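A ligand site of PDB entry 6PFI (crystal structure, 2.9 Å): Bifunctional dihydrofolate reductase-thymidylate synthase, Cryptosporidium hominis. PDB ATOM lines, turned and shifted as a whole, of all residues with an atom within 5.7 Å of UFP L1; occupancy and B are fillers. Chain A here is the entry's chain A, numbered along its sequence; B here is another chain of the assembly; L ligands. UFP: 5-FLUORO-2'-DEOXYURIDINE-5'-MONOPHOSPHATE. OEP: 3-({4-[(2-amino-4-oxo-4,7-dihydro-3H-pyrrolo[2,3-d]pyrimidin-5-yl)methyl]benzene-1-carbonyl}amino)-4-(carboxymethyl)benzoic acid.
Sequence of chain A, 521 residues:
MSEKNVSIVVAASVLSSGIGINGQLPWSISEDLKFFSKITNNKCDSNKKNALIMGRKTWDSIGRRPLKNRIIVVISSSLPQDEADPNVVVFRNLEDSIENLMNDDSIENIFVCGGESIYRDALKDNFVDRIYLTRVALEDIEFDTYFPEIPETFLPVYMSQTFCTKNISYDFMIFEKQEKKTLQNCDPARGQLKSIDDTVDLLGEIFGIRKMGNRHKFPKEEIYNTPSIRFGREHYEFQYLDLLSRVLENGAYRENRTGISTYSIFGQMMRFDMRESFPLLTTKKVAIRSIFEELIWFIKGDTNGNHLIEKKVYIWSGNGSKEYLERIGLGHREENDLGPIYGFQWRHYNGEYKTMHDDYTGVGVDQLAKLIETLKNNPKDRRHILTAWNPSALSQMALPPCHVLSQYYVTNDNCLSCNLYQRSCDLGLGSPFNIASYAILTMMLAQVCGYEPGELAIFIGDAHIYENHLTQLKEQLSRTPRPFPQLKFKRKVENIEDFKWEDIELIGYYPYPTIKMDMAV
The backbone carbonyl oxygen of Cys 425 is in hydrogen-bond range of the backbone NH of His 464, 3.2 Å away. NE2 of His 464 sits at hydrogen-bond distance from NH1 of Arg 382 of chain B (3.3 Å). The guanidinium group (NH2) of Arg 423 sits at hydrogen-bond distance from the backbone carbonyl oxygen (O) of Pro 400. A ring nitrogen (NE2) of His 464 is in hydrogen-bond range of the side-chain hydroxyl of Ser 424, 2.8 Å away. The side-chain sulfur (SG) of Cys 425 lies close to the side-chain amide oxygen (OE1) of Gln 422, 3.6 Å away. O of Arg 382 of chain B is in hydrogen-bond range of NH1 of Arg 423, 3.1 Å away. The side-chain carboxylate (OD1) of Asp 381 of chain B is in salt-bridge range of the guanidinium group (NH1) of Arg 383 of chain B, 3.2 Å away. The backbone carbonyl oxygen (O) of Asp 426 lies within hydrogen-bond range of the backbone NH (N) of Ser 431 (2.9 Å).
OH of Tyr 342 touches F5 of UFP L1 (3.9 Å). CD1 of Leu 399 touches O3P of UFP L1, at 3.9 Å. CD2 of His 403 touches O4 of UFP L1, at 3.4 Å. Cys 425 touches UFP L1 (CA to O2, 3.3 Å). CA of Gly 430 touches N3 of UFP L1, at 3.9 Å. Hydrophobic or aromatic side chains within 4 Å of UFP L1: Leu 399, His 403, His 464 and Tyr 466. The nearest printed residue that does not touch UFP L1 is Trp 316 (4.1 Å).
The backbone NH (N) of Asp 426 lies within hydrogen-bond range of an oxygen (O2) of UFP L1, at 2.8 Å. An oxygen (O3') of UFP L1 sits at hydrogen-bond distance from the side-chain hydroxyl of Tyr 466 (2.7 Å). O4' of UFP L1 sits close to SG of Cys 402, at 3.7 Å. NH1 of Arg 423 is in salt-bridge range of O2P of UFP L1 (2.6 Å). The side-chain amide oxygen (OE1) of Gln 422 lies close to an oxygen (O2) of UFP L1 (3.3 Å). OG of Ser 424 sits at hydrogen-bond distance from O2P of UFP L1 (3.0 Å). The guanidinium group of Arg 257 is in salt-bridge range of an oxygen (O1P) of UFP L1, at 3.5 Å. The guanidinium group of Arg 383 of chain B is in salt-bridge range of an oxygen (O3P) of UFP L1 (2.6 Å). An oxygen (O3') of UFP L1 lies close to a ring nitrogen (NE2) of His 464. O1 of OEP L2 sits at hydrogen-bond distance from N of Gly 430 (3.3 Å). N3 of UFP L1 lies within hydrogen-bond range of OD1 of Asn 434, at 2.9 Å. The side-chain carboxylate of Asp 426 sits at hydrogen-bond distance from a nitrogen (N2) of OEP L2, 3.4 Å away. NE of Arg 382 of chain B lies within salt-bridge range of O1P of UFP L1 (2.9 Å).
N4 of OEP L2 is in hydrogen-bond range of O3' of UFP L1 (3.4 Å).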
ATOM      1  N   ASN A 256      -6.904  25.780 -17.052  1.00  0.00           N
ATOM      2  CA  ASN A 256      -7.988  25.413 -16.146  1.00  0.00           C
ATOM      3  C   ASN A 256      -8.608  26.696 -15.606  1.00  0.00           C
ATOM      4  O   ASN A 256      -8.254  27.808 -16.031  1.00  0.00           O
ATOM      5  CB  ASN A 256      -7.487  24.501 -15.027  1.00  0.00           C
ATOM      6  CG  ASN A 256      -6.264  25.039 -14.327  1.00  0.00           C
ATOM      7  OD1 ASN A 256      -6.370  25.861 -13.413  1.00  0.00           O
ATOM      8  ND2 ASN A 256      -5.089  24.598 -14.754  1.00  0.00           N
ATOM      9  N   ARG A 257      -9.545  26.549 -14.667  1.00  0.00           N
ATOM     10  CA  ARG A 257     -10.273  27.695 -14.120  1.00  0.00           C
ATOM     11  C   ARG A 257      -9.367  28.686 -13.401  1.00  0.00           C
ATOM     12  O   ARG A 257      -9.729  29.858 -13.281  1.00  0.00           O
ATOM     13  CB  ARG A 257     -11.371  27.205 -13.178  1.00  0.00           C
ATOM     14  CG  ARG A 257     -10.855  26.292 -12.085  1.00  0.00           C
ATOM     15  CD  ARG A 257     -11.887  26.090 -10.997  1.00  0.00           C
ATOM     16  NE  ARG A 257     -11.300  25.419  -9.841  1.00  0.00           N
ATOM     17  CZ  ARG A 257     -10.657  26.042  -8.866  1.00  0.00           C
ATOM     18  NH1 ARG A 257     -10.516  27.360  -8.900  1.00  0.00           N
ATOM     19  NH2 ARG A 257     -10.142  25.351  -7.853  1.00  0.00           N
ATOM     20  N   GLU A 294      -8.823  18.859   9.377  1.00  0.00           N
ATOM     21  CA  GLU A 294      -9.754  18.911   8.246  1.00  0.00           C
ATOM     22  C   GLU A 294     -10.628  17.666   8.203  1.00  0.00           C
ATOM     23  O   GLU A 294     -11.826  17.762   7.899  1.00  0.00           O
ATOM     24  CB  GLU A 294      -8.984  19.079   6.933  1.00  0.00           C
ATOM     25  CG  GLU A 294      -9.869  19.122   5.695  1.00  0.00           C
ATOM     26  CD  GLU A 294      -9.114  18.866   4.401  1.00  0.00           C
ATOM     27  OE1 GLU A 294      -8.079  18.169   4.448  1.00  0.00           O
ATOM     28  OE2 GLU A 294      -9.556  19.349   3.343  1.00  0.00           O
ATOM     29  N   TRP A 316      -8.378  26.187   3.590  1.00  0.00           N
ATOM     30  CA  TRP A 316      -9.601  26.600   2.928  1.00  0.00           C
ATOM     31  C   TRP A 316      -9.800  28.113   2.951  1.00  0.00           C
ATOM     32  O   TRP A 316     -10.927  28.595   2.825  1.00  0.00           O
ATOM     33  CB  TRP A 316     -10.815  25.908   3.560  1.00  0.00           C
ATOM     34  CG  TRP A 316     -10.950  24.473   3.147  1.00  0.00           C
ATOM     35  CD1 TRP A 316     -10.526  23.373   3.846  1.00  0.00           C
ATOM     36  CD2 TRP A 316     -11.541  23.977   1.943  1.00  0.00           C
ATOM     37  NE1 TRP A 316     -10.826  22.228   3.149  1.00  0.00           N
ATOM     38  CE2 TRP A 316     -11.451  22.569   1.973  1.00  0.00           C
ATOM     39  CE3 TRP A 316     -12.135  24.589   0.832  1.00  0.00           C
ATOM     40  CZ2 TRP A 316     -11.928  21.764   0.945  1.00  0.00           C
ATOM     41  CZ3 TRP A 316     -12.616  23.791  -0.190  1.00  0.00           C
ATOM     42  CH2 TRP A 316     -12.515  22.393  -0.128  1.00  0.00           C
ATOM     43  N   TYR A 342     -17.928  18.633   1.490  1.00  0.00           N
ATOM     44  CA  TYR A 342     -17.565  17.487   2.310  1.00  0.00           C
ATOM     45  C   TYR A 342     -18.078  17.665   3.727  1.00  0.00           C
ATOM     46  O   TYR A 342     -17.928  18.738   4.322  1.00  0.00           O
ATOM     47  CB  TYR A 342     -16.046  17.287   2.328  1.00  0.00           C
ATOM     48  CG  TYR A 342     -15.335  17.539   1.020  1.00  0.00           C
ATOM     49  CD1 TYR A 342     -15.330  16.593   0.002  1.00  0.00           C
ATOM     50  CD2 TYR A 342     -14.603  18.706   0.819  1.00  0.00           C
ATOM     51  CE1 TYR A 342     -14.648  16.814  -1.183  1.00  0.00           C
ATOM     52  CE2 TYR A 342     -13.925  18.934  -0.361  1.00  0.00           C
ATOM     53  CZ  TYR A 342     -13.954  17.986  -1.363  1.00  0.00           C
ATOM     54  OH  TYR A 342     -13.280  18.223  -2.538  1.00  0.00           O
ATOM     55  N   LEU A 399     -16.618  24.876  -3.971  1.00  0.00           N
ATOM     56  CA  LEU A 399     -15.725  24.062  -4.794  1.00  0.00           C
ATOM     57  C   LEU A 399     -16.286  22.647  -4.852  1.00  0.00           C
ATOM     58  O   LEU A 399     -16.506  22.023  -3.810  1.00  0.00           O
ATOM     59  CB  LEU A 399     -14.300  24.069  -4.218  1.00  0.00           C
ATOM     60  CG  LEU A 399     -13.211  23.427  -5.074  1.00  0.00           C
ATOM     61  CD1 LEU A 399     -13.069  24.171  -6.395  1.00  0.00           C
ATOM     62  CD2 LEU A 399     -11.884  23.414  -4.327  1.00  0.00           C
ATOM     63  N   PRO A 400     -16.538  22.118  -6.045  1.00  0.00           N
ATOM     64  CA  PRO A 400     -17.071  20.751  -6.156  1.00  0.00           C
ATOM     65  C   PRO A 400     -16.114  19.737  -5.557  1.00  0.00           C
ATOM     66  O   PRO A 400     -14.902  19.985  -5.464  1.00  0.00           O
ATOM     67  CB  PRO A 400     -17.210  20.560  -7.673  1.00  0.00           C
ATOM     68  CG  PRO A 400     -17.425  21.931  -8.192  1.00  0.00           C
ATOM     69  CD  PRO A 400     -16.528  22.808  -7.346  1.00  0.00           C
ATOM     70  N   CYS A 402     -13.467  16.995  -4.862  1.00  0.00           N
ATOM     71  CA  CYS A 402     -12.372  16.365  -5.573  1.00  0.00           C
ATOM     72  C   CYS A 402     -12.325  14.869  -5.287  1.00  0.00           C
ATOM     73  O   CYS A 402     -12.379  14.043  -6.199  1.00  0.00           O
ATOM     74  CB  CYS A 402     -11.048  17.035  -5.208  1.00  0.00           C
ATOM     75  SG  CYS A 402     -10.968  18.745  -5.739  1.00  0.00           S
ATOM     76  N   HIS A 403     -12.232  14.507  -4.010  1.00  0.00           N
ATOM     77  CA  HIS A 403     -12.431  13.111  -3.611  1.00  0.00           C
ATOM     78  C   HIS A 403     -13.936  12.872  -3.585  1.00  0.00           C
ATOM     79  O   HIS A 403     -14.641  13.250  -2.652  1.00  0.00           O
ATOM     80  CB  HIS A 403     -11.772  12.818  -2.265  1.00  0.00           C
ATOM     81  CG  HIS A 403     -11.916  13.901  -1.243  1.00  0.00           C
ATOM     82  ND1 HIS A 403     -12.725  13.768  -0.129  1.00  0.00           N
ATOM     83  CD2 HIS A 403     -11.323  15.119  -1.138  1.00  0.00           C
ATOM     84  CE1 HIS A 403     -12.638  14.867   0.593  1.00  0.00           C
ATOM     85  NE2 HIS A 403     -11.799  15.705   0.009  1.00  0.00           N
ATOM     86  N   GLN A 422     -10.939   9.991  -7.164  1.00  0.00           N
ATOM     87  CA  GLN A 422     -10.643  11.416  -7.105  1.00  0.00           C
ATOM     88  C   GLN A 422     -10.700  11.975  -8.513  1.00  0.00           C
ATOM     89  O   GLN A 422      -9.910  11.568  -9.379  1.00  0.00           O
ATOM     90  CB  GLN A 422      -9.268  11.646  -6.474  1.00  0.00           C
ATOM     91  CG  GLN A 422      -8.962  13.075  -6.061  1.00  0.00           C
ATOM     92  CD  GLN A 422      -7.673  13.168  -5.269  1.00  0.00           C
ATOM     93  OE1 GLN A 422      -7.087  14.248  -5.138  1.00  0.00           O
ATOM     94  NE2 GLN A 422      -7.224  12.044  -4.730  1.00  0.00           N
ATOM     95  N   ARG A 423     -11.614  12.913  -8.752  1.00  0.00           N
ATOM     96  CA  ARG A 423     -11.814  13.438 -10.101  1.00  0.00           C
ATOM     97  C   ARG A 423     -10.671  14.348 -10.526  1.00  0.00           C
ATOM     98  O   ARG A 423     -10.310  14.381 -11.709  1.00  0.00           O
ATOM     99  CB  ARG A 423     -13.142  14.176 -10.195  1.00  0.00           C
ATOM    100  CG  ARG A 423     -13.255  15.382  -9.276  1.00  0.00           C
ATOM    101  CD  ARG A 423     -14.262  16.393  -9.792  1.00  0.00           C
ATOM    102  NE  ARG A 423     -14.352  17.569  -8.928  1.00  0.00           N
ATOM    103  CZ  ARG A 423     -13.547  18.628  -9.029  1.00  0.00           C
ATOM    104  NH1 ARG A 423     -12.607  18.664  -9.958  1.00  0.00           N
ATOM    105  NH2 ARG A 423     -13.707  19.647  -8.197  1.00  0.00           N
ATOM    106  N   SER A 424     -10.095  15.111  -9.594  1.00  0.00           N
ATOM    107  CA  SER A 424      -9.015  16.025  -9.898  1.00  0.00           C
ATOM    108  C   SER A 424      -8.037  16.012  -8.732  1.00  0.00           C
ATOM    109  O   SER A 424      -8.441  16.170  -7.574  1.00  0.00           O
ATOM    110  CB  SER A 424      -9.543  17.448 -10.124  1.00  0.00           C
ATOM    111  OG  SER A 424      -8.491  18.360 -10.405  1.00  0.00           O
ATOM    112  N   CYS A 425      -6.754  15.815  -9.033  1.00  0.00           N
ATOM    113  CA  CYS A 425      -5.755  15.568  -8.007  1.00  0.00           C
ATOM    114  C   CYS A 425      -4.566  16.506  -8.225  1.00  0.00           C
ATOM    115  O   CYS A 425      -3.761  16.294  -9.136  1.00  0.00           O
ATOM    116  CB  CYS A 425      -5.310  14.099  -8.028  1.00  0.00           C
ATOM    117  SG  CYS A 425      -3.969  13.696  -6.904  1.00  0.00           S
ATOM    118  N   ASP A 426      -4.459  17.520  -7.380  1.00  0.00           N
ATOM    119  CA  ASP A 426      -3.290  18.387  -7.330  1.00  0.00           C
ATOM    120  C   ASP A 426      -2.162  17.609  -6.661  1.00  0.00           C
ATOM    121  O   ASP A 426      -2.076  17.533  -5.429  1.00  0.00           O
ATOM    122  CB  ASP A 426      -3.619  19.677  -6.582  1.00  0.00           C
ATOM    123  CG  ASP A 426      -2.429  20.614  -6.466  1.00  0.00           C
ATOM    124  OD1 ASP A 426      -1.378  20.357  -7.104  1.00  0.00           O
ATOM    125  OD2 ASP A 426      -2.550  21.618  -5.737  1.00  0.00           O
ATOM    126  N   LEU A 427      -1.259  17.053  -7.471  1.00  0.00           N
ATOM    127  CA  LEU A 427      -0.206  16.177  -6.948  1.00  0.00           C
ATOM    128  C   LEU A 427       0.783  16.923  -6.052  1.00  0.00           C
ATOM    129  O   LEU A 427       1.530  16.276  -5.320  1.00  0.00           O
ATOM    130  CB  LEU A 427       0.549  15.513  -8.099  1.00  0.00           C
ATOM    131  CG  LEU A 427      -0.213  14.439  -8.879  1.00  0.00           C
ATOM    132  CD1 LEU A 427       0.617  13.949 -10.039  1.00  0.00           C
ATOM    133  CD2 LEU A 427      -0.592  13.285  -7.962  1.00  0.00           C
ATOM    134  N   GLY A 430      -2.774  18.692  -2.847  1.00  0.00           N
ATOM    135  CA  GLY A 430      -3.930  17.901  -2.435  1.00  0.00           C
ATOM    136  C   GLY A 430      -3.610  16.424  -2.285  1.00  0.00           C
ATOM    137  O   GLY A 430      -4.106  15.764  -1.376  1.00  0.00           O
ATOM    138  N   SER A 431      -2.780  15.881  -3.190  1.00  0.00           N
ATOM    139  CA  SER A 431      -2.521  14.448  -3.190  1.00  0.00           C
ATOM    140  C   SER A 431      -1.900  13.956  -1.887  1.00  0.00           C
ATOM    141  O   SER A 431      -2.427  12.991  -1.305  1.00  0.00           O
ATOM    142  CB  SER A 431      -1.663  14.072  -4.401  1.00  0.00           C
ATOM    143  OG  SER A 431      -1.547  12.668  -4.513  1.00  0.00           O
ATOM    144  N   ASN A 434      -4.693  13.934   0.574  1.00  0.00           N
ATOM    145  CA  ASN A 434      -5.725  12.921   0.359  1.00  0.00           C
ATOM    146  C   ASN A 434      -5.242  11.532   0.753  1.00  0.00           C
ATOM    147  O   ASN A 434      -6.045  10.711   1.203  1.00  0.00           O
ATOM    148  CB  ASN A 434      -6.184  12.927  -1.091  1.00  0.00           C
ATOM    149  CG  ASN A 434      -7.027  14.139  -1.433  1.00  0.00           C
ATOM    150  OD1 ASN A 434      -6.707  14.901  -2.354  1.00  0.00           O
ATOM    151  ND2 ASN A 434      -8.120  14.334  -0.693  1.00  0.00           N
ATOM    152  N   HIS A 464      -2.700  15.948 -12.116  1.00  0.00           N
ATOM    153  CA  HIS A 464      -2.030  17.068 -12.743  1.00  0.00           C
ATOM    154  C   HIS A 464      -1.033  17.700 -11.787  1.00  0.00           C
ATOM    155  O   HIS A 464      -1.115  17.558 -10.561  1.00  0.00           O
ATOM    156  CB  HIS A 464      -3.041  18.127 -13.218  1.00  0.00           C
ATOM    157  CG  HIS A 464      -4.011  18.536 -12.159  1.00  0.00           C
ATOM    158  ND1 HIS A 464      -3.686  19.425 -11.156  1.00  0.00           N
ATOM    159  CD2 HIS A 464      -5.300  18.176 -11.945  1.00  0.00           C
ATOM    160  CE1 HIS A 464      -4.737  19.593 -10.364  1.00  0.00           C
ATOM    161  NE2 HIS A 464      -5.731  18.855 -10.827  1.00  0.00           N
ATOM    162  N   TYR A 466       0.648  21.562 -11.155  1.00  0.00           N
ATOM    163  CA  TYR A 466       0.633  22.983 -11.499  1.00  0.00           C
ATOM    164  C   TYR A 466       2.033  23.447 -11.862  1.00  0.00           C
ATOM    165  O   TYR A 466       3.019  23.013 -11.271  1.00  0.00           O
ATOM    166  CB  TYR A 466       0.075  23.801 -10.333  1.00  0.00           C
ATOM    167  CG  TYR A 466      -1.421  23.704 -10.201  1.00  0.00           C
ATOM    168  CD1 TYR A 466      -2.010  22.691  -9.458  1.00  0.00           C
ATOM    169  CD2 TYR A 466      -2.251  24.609 -10.854  1.00  0.00           C
ATOM    170  CE1 TYR A 466      -3.388  22.601  -9.345  1.00  0.00           C
ATOM    171  CE2 TYR A 466      -3.625  24.511 -10.746  1.00  0.00           C
ATOM    172  CZ  TYR A 466      -4.181  23.512 -10.001  1.00  0.00           C
ATOM    173  OH  TYR A 466      -5.555  23.422  -9.904  1.00  0.00           O
ATOM    174  N   ASP B 381     -12.478  21.328 -18.736  1.00  0.00           N
ATOM    175  CA  ASP B 381     -13.064  21.302 -17.400  1.00  0.00           C
ATOM    176  C   ASP B 381     -12.816  19.958 -16.742  1.00  0.00           C
ATOM    177  O   ASP B 381     -12.874  18.906 -17.397  1.00  0.00           O
ATOM    178  CB  ASP B 381     -14.560  21.587 -17.471  1.00  0.00           C
ATOM    179  CG  ASP B 381     -15.201  21.751 -16.109  1.00  0.00           C
ATOM    180  OD1 ASP B 381     -14.598  22.411 -15.238  1.00  0.00           O
ATOM    181  OD2 ASP B 381     -16.309  21.203 -15.908  1.00  0.00           O
ATOM    182  N   ARG B 382     -12.537  19.983 -15.437  1.00  0.00           N
ATOM    183  CA  ARG B 382     -12.243  18.781 -14.664  1.00  0.00           C
ATOM    184  C   ARG B 382     -13.458  18.296 -13.876  1.00  0.00           C
ATOM    185  O   ARG B 382     -13.309  17.747 -12.784  1.00  0.00           O
ATOM    186  CB  ARG B 382     -11.067  19.040 -13.736  1.00  0.00           C
ATOM    187  CG  ARG B 382      -9.814  19.498 -14.457  1.00  0.00           C
ATOM    188  CD  ARG B 382      -8.641  19.743 -13.530  1.00  0.00           C
ATOM    189  NE  ARG B 382      -8.771  21.001 -12.799  1.00  0.00           N
ATOM    190  CZ  ARG B 382      -7.758  21.761 -12.414  1.00  0.00           C
ATOM    191  NH1 ARG B 382      -6.506  21.397 -12.701  1.00  0.00           N
ATOM    192  NH2 ARG B 382      -7.974  22.889 -11.747  1.00  0.00           N
ATOM    193  N   ARG B 383     -14.671  18.484 -14.425  1.00  0.00           N
ATOM    194  CA  ARG B 383     -15.885  18.132 -13.700  1.00  0.00           C
ATOM    195  C   ARG B 383     -16.899  17.389 -14.560  1.00  0.00           C
ATOM    196  O   ARG B 383     -18.090  17.369 -14.216  1.00  0.00           O
ATOM    197  CB  ARG B 383     -16.548  19.386 -13.129  1.00  0.00           C
ATOM    198  CG  ARG B 383     -15.687  20.182 -12.151  1.00  0.00           C
ATOM    199  CD  ARG B 383     -16.386  21.484 -11.779  1.00  0.00           C
ATOM    200  NE  ARG B 383     -15.660  22.232 -10.751  1.00  0.00           N
ATOM    201  CZ  ARG B 383     -14.833  23.245 -11.002  1.00  0.00           C
ATOM    202  NH1 ARG B 383     -14.626  23.646 -12.247  1.00  0.00           N
ATOM    203  NH2 ARG B 383     -14.235  23.861  -9.990  1.00  0.00           N
HETATM  204  N1  UFP L   1      -7.698  19.331  -4.917  1.00  0.00           N
HETATM  205  C2  UFP L   1      -7.256  18.070  -4.686  1.00  0.00           C
HETATM  206  N3  UFP L   1      -7.638  17.403  -3.583  1.00  0.00           N
HETATM  207  C4  UFP L   1      -8.465  17.959  -2.677  1.00  0.00           C
HETATM  208  C5  UFP L   1      -8.930  19.282  -2.901  1.00  0.00           C
HETATM  209  C6  UFP L   1      -8.530  19.925  -4.012  1.00  0.00           C
HETATM  210  O2  UFP L   1      -6.498  17.475  -5.449  1.00  0.00           O
HETATM  211  O4  UFP L   1      -8.801  17.348  -1.681  1.00  0.00           O
HETATM  212  F5  UFP L   1      -9.757  19.884  -2.024  1.00  0.00           F
HETATM  213  C1' UFP L   1      -7.350  20.168  -6.085  1.00  0.00           C
HETATM  214  C2' UFP L   1      -7.538  19.493  -7.461  1.00  0.00           C
HETATM  215  C3' UFP L   1      -7.468  20.744  -8.346  1.00  0.00           C
HETATM  216  C4' UFP L   1      -8.362  21.719  -7.551  1.00  0.00           C
HETATM  217  O3' UFP L   1      -6.139  21.236  -8.375  1.00  0.00           O
HETATM  218  O4' UFP L   1      -8.278  21.279  -6.164  1.00  0.00           O
HETATM  219  C5' UFP L   1      -9.816  21.677  -8.056  1.00  0.00           C
HETATM  220  O5' UFP L   1      -9.916  22.468  -9.240  1.00  0.00           O
HETATM  221  P   UFP L   1     -11.008  21.776 -10.195  1.00  0.00           P
HETATM  222  O1P UFP L   1     -10.962  22.468 -11.648  1.00  0.00           O
HETATM  223  O2P UFP L   1     -10.696  20.334 -10.338  1.00  0.00           O
HETATM  224  O3P UFP L   1     -12.482  21.932  -9.567  1.00  0.00           O
HETATM  225  C1  OEP L   2      -7.797  23.279  -3.292  1.00  0.00           C
HETATM  226  C10 OEP L   2      -4.336  23.659   0.658  1.00  0.00           C
HETATM  227  C11 OEP L   2      -3.312  22.804   1.050  1.00  0.00           C
HETATM  228  C12 OEP L   2      -3.500  21.422   0.989  1.00  0.00           C
HETATM  229  C13 OEP L   2      -4.720  20.902   0.557  1.00  0.00           C
HETATM  230  C14 OEP L   2      -1.984  23.352   1.503  1.00  0.00           C
HETATM  231  C15 OEP L   2       0.202  22.370   2.356  1.00  0.00           C
HETATM  232  C16 OEP L   2       0.658  23.125   3.443  1.00  0.00           C
HETATM  233  C17 OEP L   2       2.007  23.046   3.795  1.00  0.00           C
HETATM  234  C18 OEP L   2       2.890  22.241   3.090  1.00  0.00           C
HETATM  235  C19 OEP L   2       2.420  21.495   2.018  1.00  0.00           C
HETATM  236  C2  OEP L   2      -6.952  22.398  -2.606  1.00  0.00           C
HETATM  237  C20 OEP L   2       1.081  21.565   1.667  1.00  0.00           C
HETATM  238  C21 OEP L   2       3.330  20.604   1.228  1.00  0.00           C
HETATM  239  C22 OEP L   2      -0.237  24.027   4.248  1.00  0.00           C
HETATM  240  C23 OEP L   2      -0.083  23.748   5.720  1.00  0.00           C
HETATM  241  C3  OEP L   2      -5.702  21.993  -3.263  1.00  0.00           C
HETATM  242  C4  OEP L   2      -6.456  23.465  -5.101  1.00  0.00           C
HETATM  243  C5  OEP L   2      -7.580  22.098  -1.379  1.00  0.00           C
HETATM  244  C6  OEP L   2      -8.776  22.808  -1.352  1.00  0.00           C
HETATM  245  C7  OEP L   2      -7.072  21.209  -0.288  1.00  0.00           C
HETATM  246  C8  OEP L   2      -5.748  21.756   0.182  1.00  0.00           C
HETATM  247  C9  OEP L   2      -5.556  23.131   0.238  1.00  0.00           C
HETATM  248  N1  OEP L   2      -7.561  23.818  -4.528  1.00  0.00           N
HETATM  249  N2  OEP L   2      -5.576  22.596  -4.483  1.00  0.00           N
HETATM  250  N3  OEP L   2      -8.890  23.522  -2.528  1.00  0.00           N
HETATM  251  N4  OEP L   2      -6.079  23.959  -6.416  1.00  0.00           N
HETATM  252  N5  OEP L   2      -1.181  22.349   1.874  1.00  0.00           N
HETATM  253  O1  OEP L   2      -4.826  21.239  -2.840  1.00  0.00           O
HETATM  254  O2  OEP L   2      -1.657  24.528   1.530  1.00  0.00           O
HETATM  255  O3  OEP L   2       4.399  20.905   0.721  1.00  0.00           O
HETATM  256  O4  OEP L   2       2.788  19.360   1.141  1.00  0.00           O
HETATM  257  O5  OEP L   2      -0.842  23.117   6.446  1.00  0.00           O
HETATM  258  O6  OEP L   2       1.064  24.333   6.176  1.00  0.00           O
